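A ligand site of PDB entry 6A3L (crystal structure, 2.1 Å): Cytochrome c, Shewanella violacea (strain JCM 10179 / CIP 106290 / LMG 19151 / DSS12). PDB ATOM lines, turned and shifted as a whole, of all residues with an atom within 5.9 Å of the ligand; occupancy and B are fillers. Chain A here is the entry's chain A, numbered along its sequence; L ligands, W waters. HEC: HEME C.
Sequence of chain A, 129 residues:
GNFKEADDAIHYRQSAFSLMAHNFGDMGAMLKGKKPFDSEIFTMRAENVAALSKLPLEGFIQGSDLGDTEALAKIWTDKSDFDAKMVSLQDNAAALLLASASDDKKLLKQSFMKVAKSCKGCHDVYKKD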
ATOM      1  N   ILE A  10      15.959  -4.501 -15.340  1.00  0.00           N
ATOM      2  CA  ILE A  10      16.438  -4.853 -14.013  1.00  0.00           C
ATOM      3  C   ILE A  10      17.895  -4.424 -13.861  1.00  0.00           C
ATOM      4  O   ILE A  10      18.275  -3.800 -12.860  1.00  0.00           O
ATOM      5  CB  ILE A  10      16.255  -6.353 -13.738  1.00  0.00           C
ATOM      6  CG1 ILE A  10      14.787  -6.684 -13.574  1.00  0.00           C
ATOM      7  CG2 ILE A  10      17.017  -6.760 -12.508  1.00  0.00           C
ATOM      8  CD1 ILE A  10      14.533  -8.163 -13.369  1.00  0.00           C
ATOM      9  N   ARG A  13      18.141  -0.425 -13.454  1.00  0.00           N
ATOM     10  CA  ARG A  13      17.827   0.137 -12.133  1.00  0.00           C
ATOM     11  C   ARG A  13      18.857  -0.273 -11.077  1.00  0.00           C
ATOM     12  O   ARG A  13      19.238   0.537 -10.232  1.00  0.00           O
ATOM     13  CB  ARG A  13      16.408  -0.247 -11.712  1.00  0.00           C
ATOM     14  CG  ARG A  13      16.175  -1.725 -11.431  1.00  0.00           C
ATOM     15  CD  ARG A  13      14.728  -2.033 -11.726  1.00  0.00           C
ATOM     16  NE  ARG A  13      14.320  -3.277 -11.102  1.00  0.00           N
ATOM     17  CZ  ARG A  13      13.332  -4.049 -11.550  1.00  0.00           C
ATOM     18  NH1 ARG A  13      12.642  -3.695 -12.635  1.00  0.00           N
ATOM     19  NH2 ARG A  13      13.009  -5.166 -10.895  1.00  0.00           N
ATOM     20  N   GLN A  14      19.331  -1.524 -11.130  1.00  0.00           N
ATOM     21  CA  GLN A  14      20.339  -1.988 -10.173  1.00  0.00           C
ATOM     22  C   GLN A  14      21.635  -1.196 -10.283  1.00  0.00           C
ATOM     23  O   GLN A  14      22.249  -0.838  -9.255  1.00  0.00           O
ATOM     24  CB  GLN A  14      20.588  -3.480 -10.365  1.00  0.00           C
ATOM     25  CG  GLN A  14      19.429  -4.388  -9.945  1.00  0.00           C
ATOM     26  CD  GLN A  14      19.726  -5.869 -10.182  1.00  0.00           C
ATOM     27  OE1 GLN A  14      20.535  -6.222 -11.036  1.00  0.00           O
ATOM     28  NE2 GLN A  14      19.037  -6.734  -9.447  1.00  0.00           N
ATOM     29  N   SER A  15      22.082  -0.901 -11.499  1.00  0.00           N
ATOM     30  CA  SER A  15      23.303  -0.116 -11.644  1.00  0.00           C
ATOM     31  C   SER A  15      23.116   1.307 -11.131  1.00  0.00           C
ATOM     32  O   SER A  15      24.032   1.875 -10.542  1.00  0.00           O
ATOM     33  CB  SER A  15      23.777  -0.069 -13.098  1.00  0.00           C
ATOM     34  OG  SER A  15      24.331  -1.307 -13.435  1.00  0.00           O
ATOM     35  N   PHE A  17      21.195   2.357  -8.730  1.00  0.00           N
ATOM     36  CA  PHE A  17      21.262   2.285  -7.271  1.00  0.00           C
ATOM     37  C   PHE A  17      22.697   2.026  -6.793  1.00  0.00           C
ATOM     38  O   PHE A  17      23.177   2.669  -5.852  1.00  0.00           O
ATOM     39  CB  PHE A  17      20.328   1.195  -6.751  1.00  0.00           C
ATOM     40  CG  PHE A  17      18.858   1.510  -6.857  1.00  0.00           C
ATOM     41  CD1 PHE A  17      18.309   2.590  -6.197  1.00  0.00           C
ATOM     42  CD2 PHE A  17      18.010   0.694  -7.593  1.00  0.00           C
ATOM     43  CE1 PHE A  17      16.934   2.875  -6.275  1.00  0.00           C
ATOM     44  CE2 PHE A  17      16.635   0.973  -7.679  1.00  0.00           C
ATOM     45  CZ  PHE A  17      16.100   2.058  -7.010  1.00  0.00           C
ATOM     46  N   SER A  18      23.391   1.092  -7.432  1.00  0.00           N
ATOM     47  CA  SER A  18      24.748   0.756  -7.013  1.00  0.00           C
ATOM     48  C   SER A  18      25.688   1.964  -7.154  1.00  0.00           C
ATOM     49  O   SER A  18      26.530   2.211  -6.285  1.00  0.00           O
ATOM     50  CB  SER A  18      25.297  -0.415  -7.804  1.00  0.00           C
ATOM     51  OG  SER A  18      26.632  -0.623  -7.421  1.00  0.00           O
ATOM     52  N   MET A  20      24.658   4.959  -7.004  1.00  0.00           N
ATOM     53  CA  MET A  20      24.172   5.911  -6.016  1.00  0.00           C
ATOM     54  C   MET A  20      24.649   5.533  -4.619  1.00  0.00           C
ATOM     55  O   MET A  20      25.012   6.418  -3.819  1.00  0.00           O
ATOM     56  CB  MET A  20      22.651   5.983  -6.076  1.00  0.00           C
ATOM     57  CG  MET A  20      22.021   6.964  -5.116  1.00  0.00           C
ATOM     58  SD  MET A  20      20.375   7.392  -5.708  1.00  0.00           S
ATOM     59  CE  MET A  20      19.450   5.892  -5.441  1.00  0.00           C
ATOM     60  N   ALA A  21      24.661   4.239  -4.292  1.00  0.00           N
ATOM     61  CA  ALA A  21      25.149   3.805  -2.978  1.00  0.00           C
ATOM     62  C   ALA A  21      26.630   4.111  -2.806  1.00  0.00           C
ATOM     63  O   ALA A  21      27.061   4.503  -1.712  1.00  0.00           O
ATOM     64  CB  ALA A  21      24.916   2.306  -2.782  1.00  0.00           C
ATOM     65  N   PHE A  24      26.775   7.893  -2.199  1.00  0.00           N
ATOM     66  CA  PHE A  24      26.187   8.261  -0.917  1.00  0.00           C
ATOM     67  C   PHE A  24      27.084   7.865   0.260  1.00  0.00           C
ATOM     68  O   PHE A  24      27.292   8.662   1.183  1.00  0.00           O
ATOM     69  CB  PHE A  24      24.811   7.621  -0.764  1.00  0.00           C
ATOM     70  CG  PHE A  24      23.999   8.147   0.385  1.00  0.00           C
ATOM     71  CD1 PHE A  24      23.465   9.428   0.349  1.00  0.00           C
ATOM     72  CD2 PHE A  24      23.753   7.353   1.503  1.00  0.00           C
ATOM     73  CE1 PHE A  24      22.714   9.907   1.424  1.00  0.00           C
ATOM     74  CE2 PHE A  24      22.996   7.831   2.566  1.00  0.00           C
ATOM     75  CZ  PHE A  24      22.470   9.111   2.517  1.00  0.00           C
ATOM     76  N   VAL A  49      24.676  11.934  -6.497  1.00  0.00           N
ATOM     77  CA  VAL A  49      23.499  11.228  -5.969  1.00  0.00           C
ATOM     78  C   VAL A  49      22.227  11.854  -6.519  1.00  0.00           C
ATOM     79  O   VAL A  49      21.294  11.155  -6.907  1.00  0.00           O
ATOM     80  CB  VAL A  49      23.532  11.202  -4.433  1.00  0.00           C
ATOM     81  CG1 VAL A  49      22.199  10.684  -3.841  1.00  0.00           C
ATOM     82  CG2 VAL A  49      24.722  10.348  -3.938  1.00  0.00           C
ATOM     83  N   PHE A  60      11.679   0.366 -13.529  1.00  0.00           N
ATOM     84  CA  PHE A  60      10.623  -0.446 -12.938  1.00  0.00           C
ATOM     85  C   PHE A  60       9.442  -0.583 -13.896  1.00  0.00           C
ATOM     86  O   PHE A  60       8.295  -0.267 -13.596  1.00  0.00           O
ATOM     87  CB  PHE A  60      10.220   0.124 -11.578  1.00  0.00           C
ATOM     88  CG  PHE A  60      11.309  -0.025 -10.556  1.00  0.00           C
ATOM     89  CD1 PHE A  60      11.487  -1.234  -9.909  1.00  0.00           C
ATOM     90  CD2 PHE A  60      12.212   1.000 -10.332  1.00  0.00           C
ATOM     91  CE1 PHE A  60      12.515  -1.389  -8.999  1.00  0.00           C
ATOM     92  CE2 PHE A  60      13.220   0.853  -9.430  1.00  0.00           C
ATOM     93  CZ  PHE A  60      13.383  -0.337  -8.760  1.00  0.00           C
ATOM     94  N   ASP A  68      16.353 -12.365 -11.535  1.00  0.00           N
ATOM     95  CA  ASP A  68      17.351 -11.901 -10.573  1.00  0.00           C
ATOM     96  C   ASP A  68      17.065 -10.442 -10.255  1.00  0.00           C
ATOM     97  O   ASP A  68      17.660  -9.504 -10.786  1.00  0.00           O
ATOM     98  CB  ASP A  68      18.769 -12.065 -11.103  1.00  0.00           C
ATOM     99  CG  ASP A  68      19.806 -11.528 -10.119  1.00  0.00           C
ATOM    100  OD1 ASP A  68      20.802 -10.903 -10.543  1.00  0.00           O
ATOM    101  OD2 ASP A  68      19.565 -11.648  -8.902  1.00  0.00           O
ATOM    102  N   THR A  69      16.123 -10.255  -9.343  1.00  0.00           N
ATOM    103  CA  THR A  69      15.764  -8.947  -8.837  1.00  0.00           C
ATOM    104  C   THR A  69      15.439  -9.068  -7.358  1.00  0.00           C
ATOM    105  O   THR A  69      14.991 -10.124  -6.894  1.00  0.00           O
ATOM    106  CB  THR A  69      14.587  -8.354  -9.648  1.00  0.00           C
ATOM    107  OG1 THR A  69      14.258  -7.042  -9.157  1.00  0.00           O
ATOM    108  CG2 THR A  69      13.388  -9.272  -9.614  1.00  0.00           C
ATOM    109  N   GLU A  70      15.734  -8.011  -6.605  1.00  0.00           N
ATOM    110  CA  GLU A  70      15.320  -7.914  -5.209  1.00  0.00           C
ATOM    111  C   GLU A  70      14.065  -7.062  -5.061  1.00  0.00           C
ATOM    112  O   GLU A  70      13.683  -6.727  -3.934  1.00  0.00           O
ATOM    113  CB  GLU A  70      16.444  -7.341  -4.349  1.00  0.00           C
ATOM    114  CG  GLU A  70      17.743  -8.111  -4.369  1.00  0.00           C
ATOM    115  CD  GLU A  70      17.618  -9.456  -3.656  1.00  0.00           C
ATOM    116  OE1 GLU A  70      16.795  -9.562  -2.727  1.00  0.00           O
ATOM    117  OE2 GLU A  70      18.375 -10.385  -4.006  1.00  0.00           O
ATOM    118  N   ALA A  71      13.429  -6.714  -6.177  1.00  0.00           N
ATOM    119  CA  ALA A  71      12.215  -5.921  -6.134  1.00  0.00           C
ATOM    120  C   ALA A  71      11.016  -6.800  -5.789  1.00  0.00           C
ATOM    121  O   ALA A  71      10.786  -7.812  -6.447  1.00  0.00           O
ATOM    122  CB  ALA A  71      11.992  -5.225  -7.475  1.00  0.00           C
ATOM    123  N   LEU A  72      10.264  -6.399  -4.768  1.00  0.00           N
ATOM    124  CA  LEU A  72       9.028  -7.101  -4.422  1.00  0.00           C
ATOM    125  C   LEU A  72       7.934  -6.700  -5.409  1.00  0.00           C
ATOM    126  O   LEU A  72       7.817  -5.533  -5.782  1.00  0.00           O
ATOM    127  CB  LEU A  72       8.587  -6.757  -2.990  1.00  0.00           C
ATOM    128  CG  LEU A  72       9.433  -7.312  -1.844  1.00  0.00           C
ATOM    129  CD1 LEU A  72       9.280  -6.486  -0.579  1.00  0.00           C
ATOM    130  CD2 LEU A  72       9.075  -8.758  -1.568  1.00  0.00           C
ATOM    131  N   ILE A  75       5.601  -3.568  -5.448  1.00  0.00           N
ATOM    132  CA  ILE A  75       5.915  -2.274  -6.037  1.00  0.00           C
ATOM    133  C   ILE A  75       4.836  -1.852  -7.016  1.00  0.00           C
ATOM    134  O   ILE A  75       4.372  -0.708  -7.007  1.00  0.00           O
ATOM    135  CB  ILE A  75       7.302  -2.303  -6.724  1.00  0.00           C
ATOM    136  CG1 ILE A  75       8.428  -2.397  -5.680  1.00  0.00           C
ATOM    137  CG2 ILE A  75       7.463  -1.126  -7.709  1.00  0.00           C
ATOM    138  CD1 ILE A  75       9.798  -2.468  -6.296  1.00  0.00           C
ATOM    139  N   PHE A  82       5.053   4.053  -4.654  1.00  0.00           N
ATOM    140  CA  PHE A  82       6.473   3.816  -4.914  1.00  0.00           C
ATOM    141  C   PHE A  82       7.075   5.006  -5.664  1.00  0.00           C
ATOM    142  O   PHE A  82       8.137   5.515  -5.288  1.00  0.00           O
ATOM    143  CB  PHE A  82       6.654   2.518  -5.688  1.00  0.00           C
ATOM    144  CG  PHE A  82       8.083   2.191  -6.029  1.00  0.00           C
ATOM    145  CD1 PHE A  82       8.888   1.532  -5.121  1.00  0.00           C
ATOM    146  CD2 PHE A  82       8.606   2.495  -7.287  1.00  0.00           C
ATOM    147  CE1 PHE A  82      10.207   1.197  -5.436  1.00  0.00           C
ATOM    148  CE2 PHE A  82       9.918   2.166  -7.607  1.00  0.00           C
ATOM    149  CZ  PHE A  82      10.717   1.520  -6.696  1.00  0.00           C
ATOM    150  N   LYS A  85       7.697   7.871  -3.295  1.00  0.00           N
ATOM    151  CA  LYS A  85       8.917   7.732  -2.503  1.00  0.00           C
ATOM    152  C   LYS A  85      10.140   8.077  -3.332  1.00  0.00           C
ATOM    153  O   LYS A  85      11.079   8.721  -2.839  1.00  0.00           O
ATOM    154  CB  LYS A  85       9.022   6.300  -1.940  1.00  0.00           C
ATOM    155  CG  LYS A  85       7.903   5.947  -0.948  1.00  0.00           C
ATOM    156  CD  LYS A  85       8.048   4.534  -0.411  1.00  0.00           C
ATOM    157  CE  LYS A  85       6.998   4.236   0.643  1.00  0.00           C
ATOM    158  NZ  LYS A  85       7.087   5.177   1.791  1.00  0.00           N
ATOM    159  N   MET A  86      10.172   7.638  -4.596  1.00  0.00           N
ATOM    160  CA  MET A  86      11.284   7.967  -5.468  1.00  0.00           C
ATOM    161  C   MET A  86      11.365   9.464  -5.720  1.00  0.00           C
ATOM    162  O   MET A  86      12.462  10.045  -5.701  1.00  0.00           O
ATOM    163  CB  MET A  86      11.171   7.212  -6.799  1.00  0.00           C
ATOM    164  CG  MET A  86      12.468   7.199  -7.577  1.00  0.00           C
ATOM    165  SD  MET A  86      13.655   6.155  -6.709  1.00  0.00           S
ATOM    166  CE  MET A  86      13.091   4.532  -7.202  1.00  0.00           C
ATOM    167  N   LEU A  89      12.957  10.903  -2.805  1.00  0.00           N
ATOM    168  CA  LEU A  89      14.404  10.702  -2.813  1.00  0.00           C
ATOM    169  C   LEU A  89      15.069  11.781  -3.638  1.00  0.00           C
ATOM    170  O   LEU A  89      16.131  12.295  -3.254  1.00  0.00           O
ATOM    171  CB  LEU A  89      14.749   9.317  -3.374  1.00  0.00           C
ATOM    172  CG  LEU A  89      16.238   8.986  -3.533  1.00  0.00           C
ATOM    173  CD1 LEU A  89      16.973   8.840  -2.189  1.00  0.00           C
ATOM    174  CD2 LEU A  89      16.409   7.762  -4.364  1.00  0.00           C
ATOM    175  N   VAL A 115      17.981  12.027   3.395  1.00  0.00           N
ATOM    176  CA  VAL A 115      18.167  11.133   2.248  1.00  0.00           C
ATOM    177  C   VAL A 115      18.316   9.695   2.729  1.00  0.00           C
ATOM    178  O   VAL A 115      17.720   8.778   2.158  1.00  0.00           O
ATOM    179  CB  VAL A 115      19.391  11.565   1.403  1.00  0.00           C
ATOM    180  CG1 VAL A 115      19.590  10.577   0.265  1.00  0.00           C
ATOM    181  CG2 VAL A 115      19.230  12.967   0.873  1.00  0.00           C
ATOM    182  N   ALA A 116      19.151   9.478   3.741  1.00  0.00           N
ATOM    183  CA  ALA A 116      19.340   8.124   4.235  1.00  0.00           C
ATOM    184  C   ALA A 116      18.006   7.513   4.633  1.00  0.00           C
ATOM    185  O   ALA A 116      17.764   6.314   4.446  1.00  0.00           O
ATOM    186  CB  ALA A 116      20.323   8.110   5.413  1.00  0.00           C
ATOM    187  N   SER A 118      15.205   8.084   3.174  1.00  0.00           N
ATOM    188  CA  SER A 118      14.577   7.616   1.928  1.00  0.00           C
ATOM    189  C   SER A 118      15.077   6.242   1.530  1.00  0.00           C
ATOM    190  O   SER A 118      14.287   5.349   1.209  1.00  0.00           O
ATOM    191  CB  SER A 118      14.832   8.600   0.791  1.00  0.00           C
ATOM    192  OG  SER A 118      13.789   9.548   0.673  1.00  0.00           O
ATOM    193  N   CYS A 119      16.399   6.046   1.562  1.00  0.00           N
ATOM    194  CA  CYS A 119      16.980   4.754   1.206  1.00  0.00           C
ATOM    195  C   CYS A 119      16.388   3.635   2.052  1.00  0.00           C
ATOM    196  O   CYS A 119      15.884   2.643   1.518  1.00  0.00           O
ATOM    197  CB  CYS A 119      18.513   4.795   1.369  1.00  0.00           C
ATOM    198  SG  CYS A 119      19.395   6.159   0.586  1.00  0.00           S
ATOM    199  N   CYS A 122      12.259   3.181   1.600  1.00  0.00           N
ATOM    200  CA  CYS A 122      11.714   2.444   0.464  1.00  0.00           C
ATOM    201  C   CYS A 122      12.133   0.975   0.513  1.00  0.00           C
ATOM    202  O   CYS A 122      11.353   0.080   0.157  1.00  0.00           O
ATOM    203  CB  CYS A 122      12.161   3.124  -0.822  1.00  0.00           C
ATOM    204  SG  CYS A 122      11.527   2.398  -2.337  1.00  0.00           S
ATOM    205  N   HIS A 123      13.354   0.709   0.986  1.00  0.00           N
ATOM    206  CA  HIS A 123      13.860  -0.662   1.028  1.00  0.00           C
ATOM    207  C   HIS A 123      13.030  -1.533   1.951  1.00  0.00           C
ATOM    208  O   HIS A 123      12.742  -2.686   1.614  1.00  0.00           O
ATOM    209  CB  HIS A 123      15.317  -0.639   1.504  1.00  0.00           C
ATOM    210  CG  HIS A 123      16.267  -0.099   0.488  1.00  0.00           C
ATOM    211  ND1 HIS A 123      17.637  -0.174   0.631  1.00  0.00           N
ATOM    212  CD2 HIS A 123      16.050   0.521  -0.693  1.00  0.00           C
ATOM    213  CE1 HIS A 123      18.220   0.388  -0.406  1.00  0.00           C
ATOM    214  NE2 HIS A 123      17.282   0.823  -1.224  1.00  0.00           N
ATOM    215  N   TYR A 126       9.716  -2.314  -0.094  1.00  0.00           N
ATOM    216  CA  TYR A 126       9.696  -2.823  -1.459  1.00  0.00           C
ATOM    217  C   TYR A 126      10.924  -3.635  -1.866  1.00  0.00           C
ATOM    218  O   TYR A 126      11.060  -3.929  -3.059  1.00  0.00           O
ATOM    219  CB  TYR A 126       9.548  -1.668  -2.429  1.00  0.00           C
ATOM    220  CG  TYR A 126       8.253  -0.925  -2.326  1.00  0.00           C
ATOM    221  CD1 TYR A 126       7.070  -1.473  -2.802  1.00  0.00           C
ATOM    222  CD2 TYR A 126       8.219   0.359  -1.812  1.00  0.00           C
ATOM    223  CE1 TYR A 126       5.890  -0.781  -2.743  1.00  0.00           C
ATOM    224  CE2 TYR A 126       7.040   1.068  -1.754  1.00  0.00           C
ATOM    225  CZ  TYR A 126       5.868   0.490  -2.219  1.00  0.00           C
ATOM    226  OH  TYR A 126       4.690   1.193  -2.169  1.00  0.00           O
ATOM    227  N   LYS A 127      11.807  -4.015  -0.953  1.00  0.00           N
ATOM    228  CA  LYS A 127      12.979  -4.802  -1.280  1.00  0.00           C
ATOM    229  C   LYS A 127      12.996  -6.079  -0.437  1.00  0.00           C
ATOM    230  O   LYS A 127      12.848  -6.003   0.785  1.00  0.00           O
ATOM    231  CB  LYS A 127      14.257  -3.980  -1.048  1.00  0.00           C
ATOM    232  CG  LYS A 127      15.560  -4.553  -1.597  1.00  0.00           C
ATOM    233  CD  LYS A 127      16.717  -3.565  -1.372  1.00  0.00           C
ATOM    234  CE  LYS A 127      18.005  -4.325  -1.146  1.00  0.00           C
ATOM    235  NZ  LYS A 127      19.077  -3.562  -0.411  1.00  0.00           N
HETATM  236 FE   HEC L   1      17.616   1.341  -3.273  1.00  0.00          FE
HETATM  237  CHA HEC L   1      18.291  -1.750  -4.691  1.00  0.00           C
HETATM  238  CHB HEC L   1      20.929   1.764  -2.593  1.00  0.00           C
HETATM  239  CHC HEC L   1      17.097   4.700  -2.484  1.00  0.00           C
HETATM  240  CHD HEC L   1      14.353   1.003  -4.092  1.00  0.00           C
HETATM  241  NA  HEC L   1      19.283   0.213  -3.607  1.00  0.00           N
HETATM  242  C1A HEC L   1      19.339  -1.039  -4.169  1.00  0.00           C
HETATM  243  C2A HEC L   1      20.701  -1.479  -4.085  1.00  0.00           C
HETATM  244  C3A HEC L   1      21.429  -0.515  -3.519  1.00  0.00           C
HETATM  245  C4A HEC L   1      20.552   0.579  -3.201  1.00  0.00           C
HETATM  246  CMA HEC L   1      22.950  -0.567  -3.235  1.00  0.00           C
HETATM  247  CAA HEC L   1      21.210  -2.818  -4.611  1.00  0.00           C
HETATM  248  CBA HEC L   1      21.430  -2.614  -6.121  1.00  0.00           C
HETATM  249  CGA HEC L   1      22.199  -3.799  -6.640  1.00  0.00           C
HETATM  250  O1A HEC L   1      23.448  -3.732  -6.535  1.00  0.00           O
HETATM  251  O2A HEC L   1      21.604  -4.789  -7.118  1.00  0.00           O
HETATM  252  NB  HEC L   1      18.808   2.994  -2.698  1.00  0.00           N
HETATM  253  C1B HEC L   1      20.149   2.870  -2.380  1.00  0.00           C
HETATM  254  C2B HEC L   1      20.587   4.119  -1.768  1.00  0.00           C
HETATM  255  C3B HEC L   1      19.524   4.947  -1.707  1.00  0.00           C
HETATM  256  C4B HEC L   1      18.392   4.251  -2.308  1.00  0.00           C
HETATM  257  CMB HEC L   1      22.030   4.352  -1.278  1.00  0.00           C
HETATM  258  CAB HEC L   1      19.493   6.405  -1.163  1.00  0.00           C
HETATM  259  CBB HEC L   1      20.529   7.232  -1.350  1.00  0.00           C
HETATM  260  NC  HEC L   1      16.042   2.611  -3.323  1.00  0.00           N
HETATM  261  C1C HEC L   1      16.006   3.932  -2.901  1.00  0.00           C
HETATM  262  C2C HEC L   1      14.628   4.392  -2.962  1.00  0.00           C
HETATM  263  C3C HEC L   1      13.853   3.367  -3.383  1.00  0.00           C
HETATM  264  C4C HEC L   1      14.741   2.245  -3.629  1.00  0.00           C
HETATM  265  CMC HEC L   1      14.186   5.809  -2.544  1.00  0.00           C
HETATM  266  CAC HEC L   1      12.314   3.347  -3.612  1.00  0.00           C
HETATM  267  CBC HEC L   1      11.656   4.415  -4.059  1.00  0.00           C
HETATM  268  ND  HEC L   1      16.543  -0.107  -4.227  1.00  0.00           N
HETATM  269  C1D HEC L   1      15.180  -0.036  -4.443  1.00  0.00           C
HETATM  270  C2D HEC L   1      14.763  -1.248  -5.095  1.00  0.00           C
HETATM  271  C3D HEC L   1      15.848  -2.023  -5.259  1.00  0.00           C
HETATM  272  C4D HEC L   1      16.986  -1.318  -4.715  1.00  0.00           C
HETATM  273  CMD HEC L   1      13.298  -1.564  -5.498  1.00  0.00           C
HETATM  274  CAD HEC L   1      15.883  -3.416  -5.928  1.00  0.00           C
HETATM  275  CBD HEC L   1      16.475  -3.355  -7.350  1.00  0.00           C
HETATM  276  CGD HEC L   1      16.504  -4.733  -7.955  1.00  0.00           C
HETATM  277  O1D HEC L   1      17.274  -5.595  -7.473  1.00  0.00           O
HETATM  278  O2D HEC L   1      15.757  -4.997  -8.921  1.00  0.00           O
HETATM  279  O   HOH W   1      25.516  -2.762  -5.410  1.00  0.00           O
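Phe 17 touches the ligand.
Met 20 touches the ligand.
Ala 21 touches the ligand.
Phe 24 touches the ligand (CG to CBB, 3.99 Å).
Phe 60 touches the ligand.
N of Ala 71 touches O2D of the ligand (3.99 Å).
Ile 75 touches the ligand.
CE1 of Phe 82 touches CAC of the ligand (3.5 Å).
Lys 85 touches the ligand.
CE of Met 86 touches CBC of the ligand (3.5 Å).
Leu 89 touches the ligand.
Val 115 touches the ligand.
O of Ser 118 touches CMC of the ligand, 3.8 Å away.
Hydrophobic or aromatic side chains within 4 Å of the ligand: Phe 17, Met 20, Ala 21, Phe 24, Phe 60, Ile 75, Phe 82, Met 86, Leu 89, Val 115 and His 123.
Of the 29 residues printed, 20 come within 4 Å of the ligand.
The nearest printed residue that does not touch the ligand is Ser 18 (4.004 Å).
A carbon (CAB) of the ligand is covalently linked to the side-chain sulfur (SG) of Cys 119, 1.8 Å away.
O1D of the ligand sits at hydrogen-bond distance from NE2 of Gln 14, 2.9 Å away.
NE of Arg 13 lies within salt-bridge range of O2D of the ligand (3.1 Å).
An iron atom (FE) of the ligand is bound by a ring nitrogen (NE2) of His 123, at 2.1 Å.
The backbone NH (N) of Glu 70 sits at hydrogen-bond distance from an oxygen (O1D) of the ligand (3.0 Å).
The side-chain hydroxyl (OG1) of Thr 69 lies within hydrogen-bond range of an oxygen (O2D) of the ligand (2.5 Å).
The side-chain sulfur (SG) of Cys 122 is covalently linked to a carbon (CAC) of the ligand (1.8 Å).
Water W1 lies within hydrogen-bond range of O1A of the ligand and OG of Ser 18.
NE2 of Gln 14 sits at hydrogen-bond distance from O of Asp 68, at 3.4 Å.
N of Ala 71 lies within hydrogen-bond range of OG1 of Thr 69 (3.1 Å).
The side-chain hydroxyl (OG1) of Thr 69 sits at hydrogen-bond distance from the guanidinium group (NH2) of Arg 13 (2.8 Å).
A ring nitrogen (ND1) of His 123 sits close to the backbone carbonyl oxygen (O) of Cys 119 (3.4 Å).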
